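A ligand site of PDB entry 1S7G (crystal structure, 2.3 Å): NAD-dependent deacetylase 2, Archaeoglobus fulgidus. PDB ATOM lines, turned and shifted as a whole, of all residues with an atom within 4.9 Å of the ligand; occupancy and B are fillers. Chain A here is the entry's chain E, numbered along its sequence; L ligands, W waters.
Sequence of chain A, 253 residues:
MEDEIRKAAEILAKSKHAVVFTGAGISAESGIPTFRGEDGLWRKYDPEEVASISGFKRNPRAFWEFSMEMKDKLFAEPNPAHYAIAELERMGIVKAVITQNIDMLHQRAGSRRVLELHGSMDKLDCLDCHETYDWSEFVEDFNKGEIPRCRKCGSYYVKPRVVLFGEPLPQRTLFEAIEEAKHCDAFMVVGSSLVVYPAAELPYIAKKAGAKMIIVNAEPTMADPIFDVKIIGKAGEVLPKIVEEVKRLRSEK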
ATOM      1  N   GLY A  23      -9.218 -20.483   5.407  1.00  0.00           N
ATOM      2  CA  GLY A  23     -10.289 -21.385   5.763  1.00  0.00           C
ATOM      3  C   GLY A  23     -11.595 -20.666   5.552  1.00  0.00           C
ATOM      4  O   GLY A  23     -11.609 -19.503   5.130  1.00  0.00           O
ATOM      5  N   ALA A  24     -12.698 -21.345   5.853  1.00  0.00           N
ATOM      6  CA  ALA A  24     -14.048 -20.796   5.688  1.00  0.00           C
ATOM      7  C   ALA A  24     -14.272 -19.459   6.394  1.00  0.00           C
ATOM      8  O   ALA A  24     -15.161 -18.695   6.002  1.00  0.00           O
ATOM      9  CB  ALA A  24     -15.073 -21.827   6.165  1.00  0.00           C
ATOM     10  N   GLY A  25     -13.489 -19.173   7.430  1.00  0.00           N
ATOM     11  CA  GLY A  25     -13.666 -17.939   8.166  1.00  0.00           C
ATOM     12  C   GLY A  25     -13.422 -16.652   7.388  1.00  0.00           C
ATOM     13  O   GLY A  25     -14.034 -15.628   7.684  1.00  0.00           O
ATOM     14  N   ILE A  26     -12.530 -16.700   6.403  1.00  0.00           N
ATOM     15  CA  ILE A  26     -12.220 -15.510   5.612  1.00  0.00           C
ATOM     16  C   ILE A  26     -13.376 -15.129   4.689  1.00  0.00           C
ATOM     17  O   ILE A  26     -13.367 -14.043   4.091  1.00  0.00           O
ATOM     18  CB  ILE A  26     -10.953 -15.733   4.754  1.00  0.00           C
ATOM     19  CG1 ILE A  26     -10.401 -14.378   4.296  1.00  0.00           C
ATOM     20  CG2 ILE A  26     -11.288 -16.598   3.542  1.00  0.00           C
ATOM     21  CD1 ILE A  26      -9.117 -14.470   3.499  1.00  0.00           C
ATOM     22  N   ALA A  28     -16.593 -15.383   5.854  1.00  0.00           N
ATOM     23  CA  ALA A  28     -17.720 -15.128   6.751  1.00  0.00           C
ATOM     24  C   ALA A  28     -18.325 -13.770   6.365  1.00  0.00           C
ATOM     25  O   ALA A  28     -19.548 -13.635   6.280  1.00  0.00           O
ATOM     26  CB  ALA A  28     -17.234 -15.089   8.204  1.00  0.00           C
ATOM     27  N   GLU A  29     -17.454 -12.803   6.117  1.00  0.00           N
ATOM     28  CA  GLU A  29     -17.854 -11.452   5.724  1.00  0.00           C
ATOM     29  C   GLU A  29     -18.662 -11.431   4.433  1.00  0.00           C
ATOM     30  O   GLU A  29     -19.293 -10.426   4.107  1.00  0.00           O
ATOM     31  CB  GLU A  29     -16.606 -10.570   5.522  1.00  0.00           C
ATOM     32  CG  GLU A  29     -16.245  -9.630   6.669  1.00  0.00           C
ATOM     33  CD  GLU A  29     -15.805 -10.351   7.935  1.00  0.00           C
ATOM     34  OE1 GLU A  29     -14.944  -9.798   8.649  1.00  0.00           O
ATOM     35  OE2 GLU A  29     -16.326 -11.455   8.220  1.00  0.00           O
ATOM     36  N   THR A  34     -19.545 -20.505   8.334  1.00  0.00           N
ATOM     37  CA  THR A  34     -18.379 -21.343   8.599  1.00  0.00           C
ATOM     38  C   THR A  34     -18.876 -22.760   8.886  1.00  0.00           C
ATOM     39  O   THR A  34     -20.071 -23.027   8.807  1.00  0.00           O
ATOM     40  CB  THR A  34     -17.579 -20.831   9.804  1.00  0.00           C
ATOM     41  OG1 THR A  34     -18.429 -20.730  10.952  1.00  0.00           O
ATOM     42  CG2 THR A  34     -16.985 -19.467   9.507  1.00  0.00           C
ATOM     43  N   PHE A  35     -17.957 -23.655   9.215  1.00  0.00           N
ATOM     44  CA  PHE A  35     -18.319 -25.038   9.503  1.00  0.00           C
ATOM     45  C   PHE A  35     -18.263 -25.348  10.992  1.00  0.00           C
ATOM     46  O   PHE A  35     -19.140 -26.038  11.532  1.00  0.00           O
ATOM     47  CB  PHE A  35     -17.397 -25.987   8.729  1.00  0.00           C
ATOM     48  CG  PHE A  35     -17.512 -25.871   7.235  1.00  0.00           C
ATOM     49  CD1 PHE A  35     -18.573 -26.453   6.551  1.00  0.00           C
ATOM     50  CD2 PHE A  35     -16.561 -25.148   6.513  1.00  0.00           C
ATOM     51  CE1 PHE A  35     -18.688 -26.325   5.174  1.00  0.00           C
ATOM     52  CE2 PHE A  35     -16.665 -25.020   5.126  1.00  0.00           C
ATOM     53  CZ  PHE A  35     -17.733 -25.619   4.456  1.00  0.00           C
ATOM     54  N   ARG A  36     -17.234 -24.845  11.661  1.00  0.00           N
ATOM     55  CA  ARG A  36     -17.058 -25.081  13.083  1.00  0.00           C
ATOM     56  C   ARG A  36     -16.994 -23.747  13.834  1.00  0.00           C
ATOM     57  O   ARG A  36     -17.031 -22.681  13.228  1.00  0.00           O
ATOM     58  CB  ARG A  36     -15.785 -25.888  13.319  1.00  0.00           C
ATOM     59  CG  ARG A  36     -15.739 -27.189  12.522  1.00  0.00           C
ATOM     60  CD  ARG A  36     -14.461 -27.969  12.764  1.00  0.00           C
ATOM     61  NE  ARG A  36     -14.398 -29.170  11.934  1.00  0.00           N
ATOM     62  CZ  ARG A  36     -14.301 -29.172  10.609  1.00  0.00           C
ATOM     63  NH1 ARG A  36     -14.242 -30.318   9.943  1.00  0.00           N
ATOM     64  NH2 ARG A  36     -14.262 -28.017   9.940  1.00  0.00           N
ATOM     65  N   GLY A  37     -16.903 -23.822  15.155  1.00  0.00           N
ATOM     66  CA  GLY A  37     -16.858 -22.610  15.947  1.00  0.00           C
ATOM     67  C   GLY A  37     -18.252 -22.067  16.227  1.00  0.00           C
ATOM     68  O   GLY A  37     -19.153 -22.823  16.581  1.00  0.00           O
ATOM     69  N   GLU A  38     -18.420 -20.753  16.058  1.00  0.00           N
ATOM     70  CA  GLU A  38     -19.710 -20.119  16.306  1.00  0.00           C
ATOM     71  C   GLU A  38     -20.620 -20.173  15.080  1.00  0.00           C
ATOM     72  O   GLU A  38     -20.212 -19.828  13.967  1.00  0.00           O
ATOM     73  CB  GLU A  38     -19.509 -18.675  16.735  1.00  0.00           C
ATOM     74  N   TRP A  42     -21.562 -27.584  11.052  1.00  0.00           N
ATOM     75  CA  TRP A  42     -21.401 -28.915  11.656  1.00  0.00           C
ATOM     76  C   TRP A  42     -22.040 -29.012  13.044  1.00  0.00           C
ATOM     77  O   TRP A  42     -21.650 -29.843  13.865  1.00  0.00           O
ATOM     78  CB  TRP A  42     -19.916 -29.291  11.720  1.00  0.00           C
ATOM     79  CG  TRP A  42     -19.276 -29.583  10.369  1.00  0.00           C
ATOM     80  CD1 TRP A  42     -17.950 -29.785  10.124  1.00  0.00           C
ATOM     81  CD2 TRP A  42     -19.942 -29.730   9.095  1.00  0.00           C
ATOM     82  NE1 TRP A  42     -17.738 -30.042   8.796  1.00  0.00           N
ATOM     83  CE2 TRP A  42     -18.951 -30.015   8.142  1.00  0.00           C
ATOM     84  CE3 TRP A  42     -21.284 -29.643   8.680  1.00  0.00           C
ATOM     85  CZ2 TRP A  42     -19.242 -30.220   6.787  1.00  0.00           C
ATOM     86  CZ3 TRP A  42     -21.569 -29.850   7.331  1.00  0.00           C
ATOM     87  CH2 TRP A  42     -20.556 -30.130   6.402  1.00  0.00           C
ATOM     88  N   GLN A 100      -8.909 -23.827   1.484  1.00  0.00           N
ATOM     89  CA  GLN A 100      -9.697 -25.030   1.737  1.00  0.00           C
ATOM     90  C   GLN A 100     -11.136 -24.770   1.279  1.00  0.00           C
ATOM     91  O   GLN A 100     -11.960 -25.680   1.253  1.00  0.00           O
ATOM     92  CB  GLN A 100      -9.684 -25.355   3.232  1.00  0.00           C
ATOM     93  CG  GLN A 100      -8.298 -25.536   3.811  1.00  0.00           C
ATOM     94  CD  GLN A 100      -8.313 -25.732   5.308  1.00  0.00           C
ATOM     95  OE1 GLN A 100      -8.690 -26.792   5.816  1.00  0.00           O
ATOM     96  NE2 GLN A 100      -7.920 -24.702   6.039  1.00  0.00           N
ATOM     97  N   ASN A 101     -11.429 -23.519   0.920  1.00  0.00           N
ATOM     98  CA  ASN A 101     -12.769 -23.125   0.477  1.00  0.00           C
ATOM     99  C   ASN A 101     -13.035 -23.460  -0.978  1.00  0.00           C
ATOM    100  O   ASN A 101     -12.109 -23.621  -1.770  1.00  0.00           O
ATOM    101  CB  ASN A 101     -12.978 -21.621   0.656  1.00  0.00           C
ATOM    102  CG  ASN A 101     -12.670 -21.150   2.054  1.00  0.00           C
ATOM    103  OD1 ASN A 101     -13.026 -21.799   3.033  1.00  0.00           O
ATOM    104  ND2 ASN A 101     -12.023 -19.995   2.151  1.00  0.00           N
ATOM    105  N   HIS A 118      -9.040 -28.314  -1.412  1.00  0.00           N
ATOM    106  CA  HIS A 118     -10.212 -29.162  -1.295  1.00  0.00           C
ATOM    107  C   HIS A 118     -11.093 -29.186  -2.551  1.00  0.00           C
ATOM    108  O   HIS A 118     -12.296 -29.427  -2.471  1.00  0.00           O
ATOM    109  CB  HIS A 118     -11.043 -28.726  -0.079  1.00  0.00           C
ATOM    110  CG  HIS A 118     -10.394 -29.040   1.233  1.00  0.00           C
ATOM    111  ND1 HIS A 118     -10.860 -28.548   2.431  1.00  0.00           N
ATOM    112  CD2 HIS A 118      -9.310 -29.797   1.534  1.00  0.00           C
ATOM    113  CE1 HIS A 118     -10.085 -28.967   3.407  1.00  0.00           C
ATOM    114  NE2 HIS A 118      -9.139 -29.726   2.893  1.00  0.00           N
ATOM    115  N   VAL A 163     -13.452 -32.274  -2.149  1.00  0.00           N
ATOM    116  CA  VAL A 163     -13.017 -33.286  -1.199  1.00  0.00           C
ATOM    117  C   VAL A 163     -14.018 -33.461  -0.072  1.00  0.00           C
ATOM    118  O   VAL A 163     -14.217 -32.553   0.730  1.00  0.00           O
ATOM    119  CB  VAL A 163     -11.654 -32.915  -0.574  1.00  0.00           C
ATOM    120  CG1 VAL A 163     -11.284 -33.901   0.516  1.00  0.00           C
ATOM    121  CG2 VAL A 163     -10.578 -32.883  -1.641  1.00  0.00           C
ATOM    122  N   PHE A 165     -15.442 -35.982   3.242  1.00  0.00           N
ATOM    123  CA  PHE A 165     -14.789 -36.810   4.246  1.00  0.00           C
ATOM    124  C   PHE A 165     -14.601 -38.225   3.698  1.00  0.00           C
ATOM    125  O   PHE A 165     -15.478 -38.760   3.019  1.00  0.00           O
ATOM    126  CB  PHE A 165     -15.614 -36.859   5.526  1.00  0.00           C
ATOM    127  CG  PHE A 165     -15.368 -35.697   6.453  1.00  0.00           C
ATOM    128  CD1 PHE A 165     -14.099 -35.472   6.982  1.00  0.00           C
ATOM    129  CD2 PHE A 165     -16.409 -34.827   6.801  1.00  0.00           C
ATOM    130  CE1 PHE A 165     -13.863 -34.400   7.857  1.00  0.00           C
ATOM    131  CE2 PHE A 165     -16.181 -33.767   7.665  1.00  0.00           C
ATOM    132  CZ  PHE A 165     -14.908 -33.548   8.188  1.00  0.00           C
ATOM    133  N   GLY A 191      -8.849 -17.381   9.097  1.00  0.00           N
ATOM    134  CA  GLY A 191     -10.144 -18.005   9.229  1.00  0.00           C
ATOM    135  C   GLY A 191     -10.148 -19.518   9.100  1.00  0.00           C
ATOM    136  O   GLY A 191     -10.954 -20.075   8.362  1.00  0.00           O
ATOM    137  N   SER A 192      -9.244 -20.178   9.826  1.00  0.00           N
ATOM    138  CA  SER A 192      -9.149 -21.625   9.786  1.00  0.00           C
ATOM    139  C   SER A 192      -9.061 -22.249  11.170  1.00  0.00           C
ATOM    140  O   SER A 192      -8.200 -21.899  11.977  1.00  0.00           O
ATOM    141  CB  SER A 192      -7.945 -22.054   8.950  1.00  0.00           C
ATOM    142  OG  SER A 192      -7.839 -23.467   8.913  1.00  0.00           O
ATOM    143  N   SER A 193      -9.961 -23.193  11.439  1.00  0.00           N
ATOM    144  CA  SER A 193     -10.004 -23.889  12.720  1.00  0.00           C
ATOM    145  C   SER A 193      -8.765 -24.796  12.865  1.00  0.00           C
ATOM    146  O   SER A 193      -8.365 -25.131  13.975  1.00  0.00           O
ATOM    147  CB  SER A 193     -11.286 -24.725  12.801  1.00  0.00           C
ATOM    148  OG  SER A 193     -11.495 -25.221  14.112  1.00  0.00           O
ATOM    149  N   LEU A 194      -8.191 -25.181  11.735  1.00  0.00           N
ATOM    150  CA  LEU A 194      -7.003 -26.045  11.718  1.00  0.00           C
ATOM    151  C   LEU A 194      -7.224 -27.387  12.427  1.00  0.00           C
ATOM    152  O   LEU A 194      -6.397 -27.818  13.238  1.00  0.00           O
ATOM    153  CB  LEU A 194      -5.799 -25.321  12.339  1.00  0.00           C
ATOM    154  CG  LEU A 194      -5.268 -24.080  11.604  1.00  0.00           C
ATOM    155  CD1 LEU A 194      -4.040 -23.521  12.324  1.00  0.00           C
ATOM    156  CD2 LEU A 194      -4.887 -24.456  10.177  1.00  0.00           C
ATOM    157  N   VAL A 195      -8.332 -28.048  12.122  1.00  0.00           N
ATOM    158  CA  VAL A 195      -8.650 -29.341  12.713  1.00  0.00           C
ATOM    159  C   VAL A 195      -8.699 -30.435  11.645  1.00  0.00           C
ATOM    160  O   VAL A 195      -8.455 -31.598  11.941  1.00  0.00           O
ATOM    161  CB  VAL A 195     -10.013 -29.333  13.452  1.00  0.00           C
ATOM    162  CG1 VAL A 195      -9.990 -28.304  14.575  1.00  0.00           C
ATOM    163  CG2 VAL A 195     -11.147 -29.026  12.479  1.00  0.00           C
ATOM    164  N   VAL A 196      -9.011 -30.057  10.400  1.00  0.00           N
ATOM    165  CA  VAL A 196      -9.068 -31.045   9.324  1.00  0.00           C
ATOM    166  C   VAL A 196      -7.712 -31.263   8.680  1.00  0.00           C
ATOM    167  O   VAL A 196      -7.071 -30.334   8.178  1.00  0.00           O
ATOM    168  CB  VAL A 196     -10.100 -30.649   8.222  1.00  0.00           C
ATOM    169  CG1 VAL A 196      -9.794 -29.266   7.704  1.00  0.00           C
ATOM    170  CG2 VAL A 196     -10.050 -31.651   7.086  1.00  0.00           C
ATOM    171  N   VAL A 216      -4.728 -15.203  11.817  1.00  0.00           N
ATOM    172  CA  VAL A 216      -5.832 -14.289  12.043  1.00  0.00           C
ATOM    173  C   VAL A 216      -7.112 -15.107  12.073  1.00  0.00           C
ATOM    174  O   VAL A 216      -7.575 -15.577  11.041  1.00  0.00           O
ATOM    175  CB  VAL A 216      -5.912 -13.250  10.905  1.00  0.00           C
ATOM    176  CG1 VAL A 216      -7.057 -12.283  11.159  1.00  0.00           C
ATOM    177  CG2 VAL A 216      -4.596 -12.507  10.786  1.00  0.00           C
ATOM    178  N   ASN A 217      -7.685 -15.277  13.261  1.00  0.00           N
ATOM    179  CA  ASN A 217      -8.923 -16.048  13.412  1.00  0.00           C
ATOM    180  C   ASN A 217      -9.824 -15.428  14.479  1.00  0.00           C
ATOM    181  O   ASN A 217      -9.348 -14.854  15.454  1.00  0.00           O
ATOM    182  CB  ASN A 217      -8.602 -17.501  13.768  1.00  0.00           C
ATOM    183  CG  ASN A 217      -9.698 -18.468  13.337  1.00  0.00           C
ATOM    184  OD1 ASN A 217      -9.895 -18.710  12.148  1.00  0.00           O
ATOM    185  ND2 ASN A 217     -10.429 -19.017  14.303  1.00  0.00           N
ATOM    186  N   ALA A 218     -11.133 -15.580  14.296  1.00  0.00           N
ATOM    187  CA  ALA A 218     -12.122 -15.028  15.234  1.00  0.00           C
ATOM    188  C   ALA A 218     -12.066 -15.667  16.614  1.00  0.00           C
ATOM    189  O   ALA A 218     -12.821 -15.295  17.512  1.00  0.00           O
ATOM    190  CB  ALA A 218     -13.526 -15.165  14.652  1.00  0.00           C
ATOM    191  N   GLU A 219     -11.175 -16.641  16.785  1.00  0.00           N
ATOM    192  CA  GLU A 219     -11.026 -17.313  18.067  1.00  0.00           C
ATOM    193  C   GLU A 219      -9.738 -18.136  18.088  1.00  0.00           C
ATOM    194  O   GLU A 219      -9.194 -18.482  17.041  1.00  0.00           O
ATOM    195  CB  GLU A 219     -12.243 -18.207  18.335  1.00  0.00           C
ATOM    196  CG  GLU A 219     -12.480 -19.315  17.322  1.00  0.00           C
ATOM    197  CD  GLU A 219     -13.893 -19.884  17.399  1.00  0.00           C
ATOM    198  OE1 GLU A 219     -14.152 -20.917  16.742  1.00  0.00           O
ATOM    199  OE2 GLU A 219     -14.744 -19.290  18.088  1.00  0.00           O
ATOM    200  N   GLY A 233      -9.591 -11.790  15.814  1.00  0.00           N
ATOM    201  CA  GLY A 233     -10.564 -10.845  15.300  1.00  0.00           C
ATOM    202  C   GLY A 233     -11.150 -11.321  13.985  1.00  0.00           C
ATOM    203  O   GLY A 233     -10.960 -12.466  13.579  1.00  0.00           O
ATOM    204  N   LYS A 234     -11.882 -10.431  13.315  1.00  0.00           N
ATOM    205  CA  LYS A 234     -12.504 -10.753  12.034  1.00  0.00           C
ATOM    206  C   LYS A 234     -11.556 -10.395  10.884  1.00  0.00           C
ATOM    207  O   LYS A 234     -10.996  -9.308  10.852  1.00  0.00           O
ATOM    208  CB  LYS A 234     -13.825 -10.011  11.902  1.00  0.00           C
ATOM    209  CG  LYS A 234     -14.853 -10.415  12.953  1.00  0.00           C
ATOM    210  CD  LYS A 234     -16.093  -9.540  12.923  1.00  0.00           C
ATOM    211  CE  LYS A 234     -16.816  -9.619  11.587  1.00  0.00           C
ATOM    212  NZ  LYS A 234     -18.042  -8.769  11.562  1.00  0.00           N
ATOM    213  N   ALA A 235     -11.409 -11.332   9.950  1.00  0.00           N
ATOM    214  CA  ALA A 235     -10.531 -11.158   8.794  1.00  0.00           C
ATOM    215  C   ALA A 235     -10.864  -9.949   7.937  1.00  0.00           C
ATOM    216  O   ALA A 235      -9.964  -9.307   7.400  1.00  0.00           O
ATOM    217  CB  ALA A 235     -10.557 -12.418   7.938  1.00  0.00           C
ATOM    218  N   GLY A 236     -12.151  -9.645   7.805  1.00  0.00           N
ATOM    219  CA  GLY A 236     -12.553  -8.507   6.998  1.00  0.00           C
ATOM    220  C   GLY A 236     -12.102  -7.174   7.564  1.00  0.00           C
ATOM    221  O   GLY A 236     -12.018  -6.187   6.848  1.00  0.00           O
HETATM  222  N1  LIG L   1     -12.682 -13.747  10.274  1.00  0.00           N
HETATM  223  C1  LIG L   1     -11.708 -14.666  10.600  1.00  0.00           C
HETATM  224  N2  LIG L   1     -12.122 -15.952  11.169  1.00  0.00           N
HETATM  225  C2  LIG L   1     -13.544 -16.203  11.345  1.00  0.00           C
HETATM  226  C3  LIG L   1     -14.592 -15.252  11.000  1.00  0.00           C
HETATM  227  C4  LIG L   1     -14.130 -13.914  10.421  1.00  0.00           C
HETATM  228  N3  LIG L   1     -14.974 -12.979  10.081  1.00  0.00           N
HETATM  229  N4  LIG L   1     -15.773 -15.787  11.271  1.00  0.00           N
HETATM  230  C5  LIG L   1     -15.532 -17.007  11.773  1.00  0.00           C
HETATM  231  N5  LIG L   1     -14.160 -17.359  11.851  1.00  0.00           N
HETATM  232  C6  LIG L   1     -13.384 -18.540  12.302  1.00  0.00           C
HETATM  233  C7  LIG L   1     -14.131 -19.522  13.245  1.00  0.00           C
HETATM  234  O1  LIG L   1     -14.186 -19.114  14.558  1.00  0.00           O
HETATM  235  C8  LIG L   1     -13.412 -20.832  12.927  1.00  0.00           C
HETATM  236  O2  LIG L   1     -12.327 -21.167  13.835  1.00  0.00           O
HETATM  237  O3  LIG L   1     -13.050 -19.261  11.124  1.00  0.00           O
HETATM  238  C9  LIG L   1     -12.730 -20.636  11.523  1.00  0.00           C
HETATM  239  C10 LIG L   1     -13.267 -21.494  10.414  1.00  0.00           C
HETATM  240  O4  LIG L   1     -13.050 -22.902  10.783  1.00  0.00           O
HETATM  241  P1  LIG L   1     -13.931 -24.049  10.187  1.00  0.00           P
HETATM  242  O5  LIG L   1     -13.516 -25.313  10.850  1.00  0.00           O
HETATM  243  O6  LIG L   1     -15.320 -23.718  10.186  1.00  0.00           O
HETATM  244  O7  LIG L   1     -13.408 -24.094   8.668  1.00  0.00           O
HETATM  245  P2  LIG L   1     -12.015 -24.559   7.913  1.00  0.00           P
HETATM  246  O8  LIG L   1     -10.780 -24.279   8.732  1.00  0.00           O
HETATM  247  O9  LIG L   1     -12.095 -23.940   6.506  1.00  0.00           O
HETATM  248  O10 LIG L   1     -12.032 -26.213   7.800  1.00  0.00           O
HETATM  249  C11 LIG L   1     -13.181 -26.726   7.180  1.00  0.00           C
HETATM  250  O11 LIG L   1     -14.043 -28.834   6.950  1.00  0.00           O
HETATM  251  O12 LIG L   1     -15.371 -30.589   6.210  1.00  0.00           O
HETATM  252  C12 LIG L   1     -15.177 -29.164   6.105  1.00  0.00           C
HETATM  253  O13 LIG L   1     -14.269 -29.640   3.836  1.00  0.00           O
HETATM  254  C13 LIG L   1     -14.775 -28.647   4.670  1.00  0.00           C
HETATM  255  O14 LIG L   1     -12.770 -27.217   3.941  1.00  0.00           O
HETATM  256  C14 LIG L   1     -13.775 -27.481   4.967  1.00  0.00           C
HETATM  257  C15 LIG L   1     -13.116 -27.876   6.310  1.00  0.00           C
HETATM  258  O   HOH W   1     -14.989 -13.158   6.841  1.00  0.00           O
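O6 of the ligand sits at hydrogen-bond distance from N of Arg 36 (2.7 Å).
O5 of the ligand lies within salt-bridge range of NH2 of Arg 36.
The backbone NH (N) of Ala 24 lies within hydrogen-bond range of an oxygen (O9) of the ligand (2.7 Å).
N of Ala 235 is in hydrogen-bond range of N1 of the ligand (2.7 Å).
The side-chain carboxylate (OE2) of Glu 29 is in hydrogen-bond range of a nitrogen (N3) of the ligand, at 2.8 Å.
ND1 of His 118 is in hydrogen-bond range of O14 of the ligand, 2.8 Å away.
O6 of the ligand sits at hydrogen-bond distance from N of Phe 35 (2.8 Å).
An oxygen (O1) of the ligand is in hydrogen-bond range of the side-chain carboxylate of Glu 219, 2.8 Å away.
The side-chain amide nitrogen of Asn 217 sits at hydrogen-bond distance from an oxygen (O2) of the ligand, at 2.9 Å.
The backbone NH (N) of Ser 193 lies within hydrogen-bond range of an oxygen (O8) of the ligand (3.0 Å).
OG of Ser 192 sits at hydrogen-bond distance from O8 of the ligand (3.1 Å).
An oxygen (O14) of the ligand is in hydrogen-bond range of the backbone carbonyl oxygen (O) of Gln 100 (3.2 Å).
The backbone NH (N) of Ala 218 sits at hydrogen-bond distance from a nitrogen (N2) of the ligand (3.3 Å).
The backbone NH (N) of Ala 24 is in hydrogen-bond range of the backbone carbonyl oxygen (O) of Gly 191, 3.3 Å away.
N of Gly 236 lies within hydrogen-bond range of OE1 of Glu 29, 2.9 Å away.
The backbone carbonyl oxygen (O) of Glu 219 sits at hydrogen-bond distance from the side-chain amide nitrogen (ND2) of Asn 217 (3.1 Å).
N of Ser 192 lies within hydrogen-bond range of OD1 of Asn 217 (2.8 Å).
The side-chain amide oxygen of Asn 217 lies close to the backbone NH of Gly 191, 3.5 Å away.
The side-chain amide nitrogen (NE2) of Gln 100 lies within hydrogen-bond range of the side-chain hydroxyl (OG) of Ser 192 (3.1 Å).
OG of Ser 192 lies close to N of Leu 194.
The side-chain amide nitrogen of Asn 101 is in hydrogen-bond range of the backbone carbonyl oxygen of Gly 23, at 3.0 Å.
N1 of the ligand sits close to O of Gly 25, at 3.5 Å.
Merely in contact with the ligand: Gly 23 (3.2 Å), Ala 28 (3.5 Å), Thr 34 (3.6 Å), Trp 42 (3.5 Å), Phe 165 (3.6 Å), Gly 191 (3.4 Å), Val 196 (3.8 Å), Gly 233 (3.8 Å) and Lys 234 (3.5 Å).
Hydrophobic or aromatic side chains within 4 Å of the ligand: Ala 24, Ala 28, Phe 35, Trp 42, His 118, Phe 165, Val 196, Ala 218 and Ala 235.
22 residues have an atom within 4 Å of the ligand: Gly 23, Ala 24, Gly 25, Ala 28, Glu 29, Thr 34, Phe 35, Arg 36, Trp 42, Gln 100, His 118, Phe 165, Gly 191, Ser 192, Ser 193, Val 196, Asn 217, Ala 218, Glu 219, Gly 233, Lys 234 and Ala 235.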
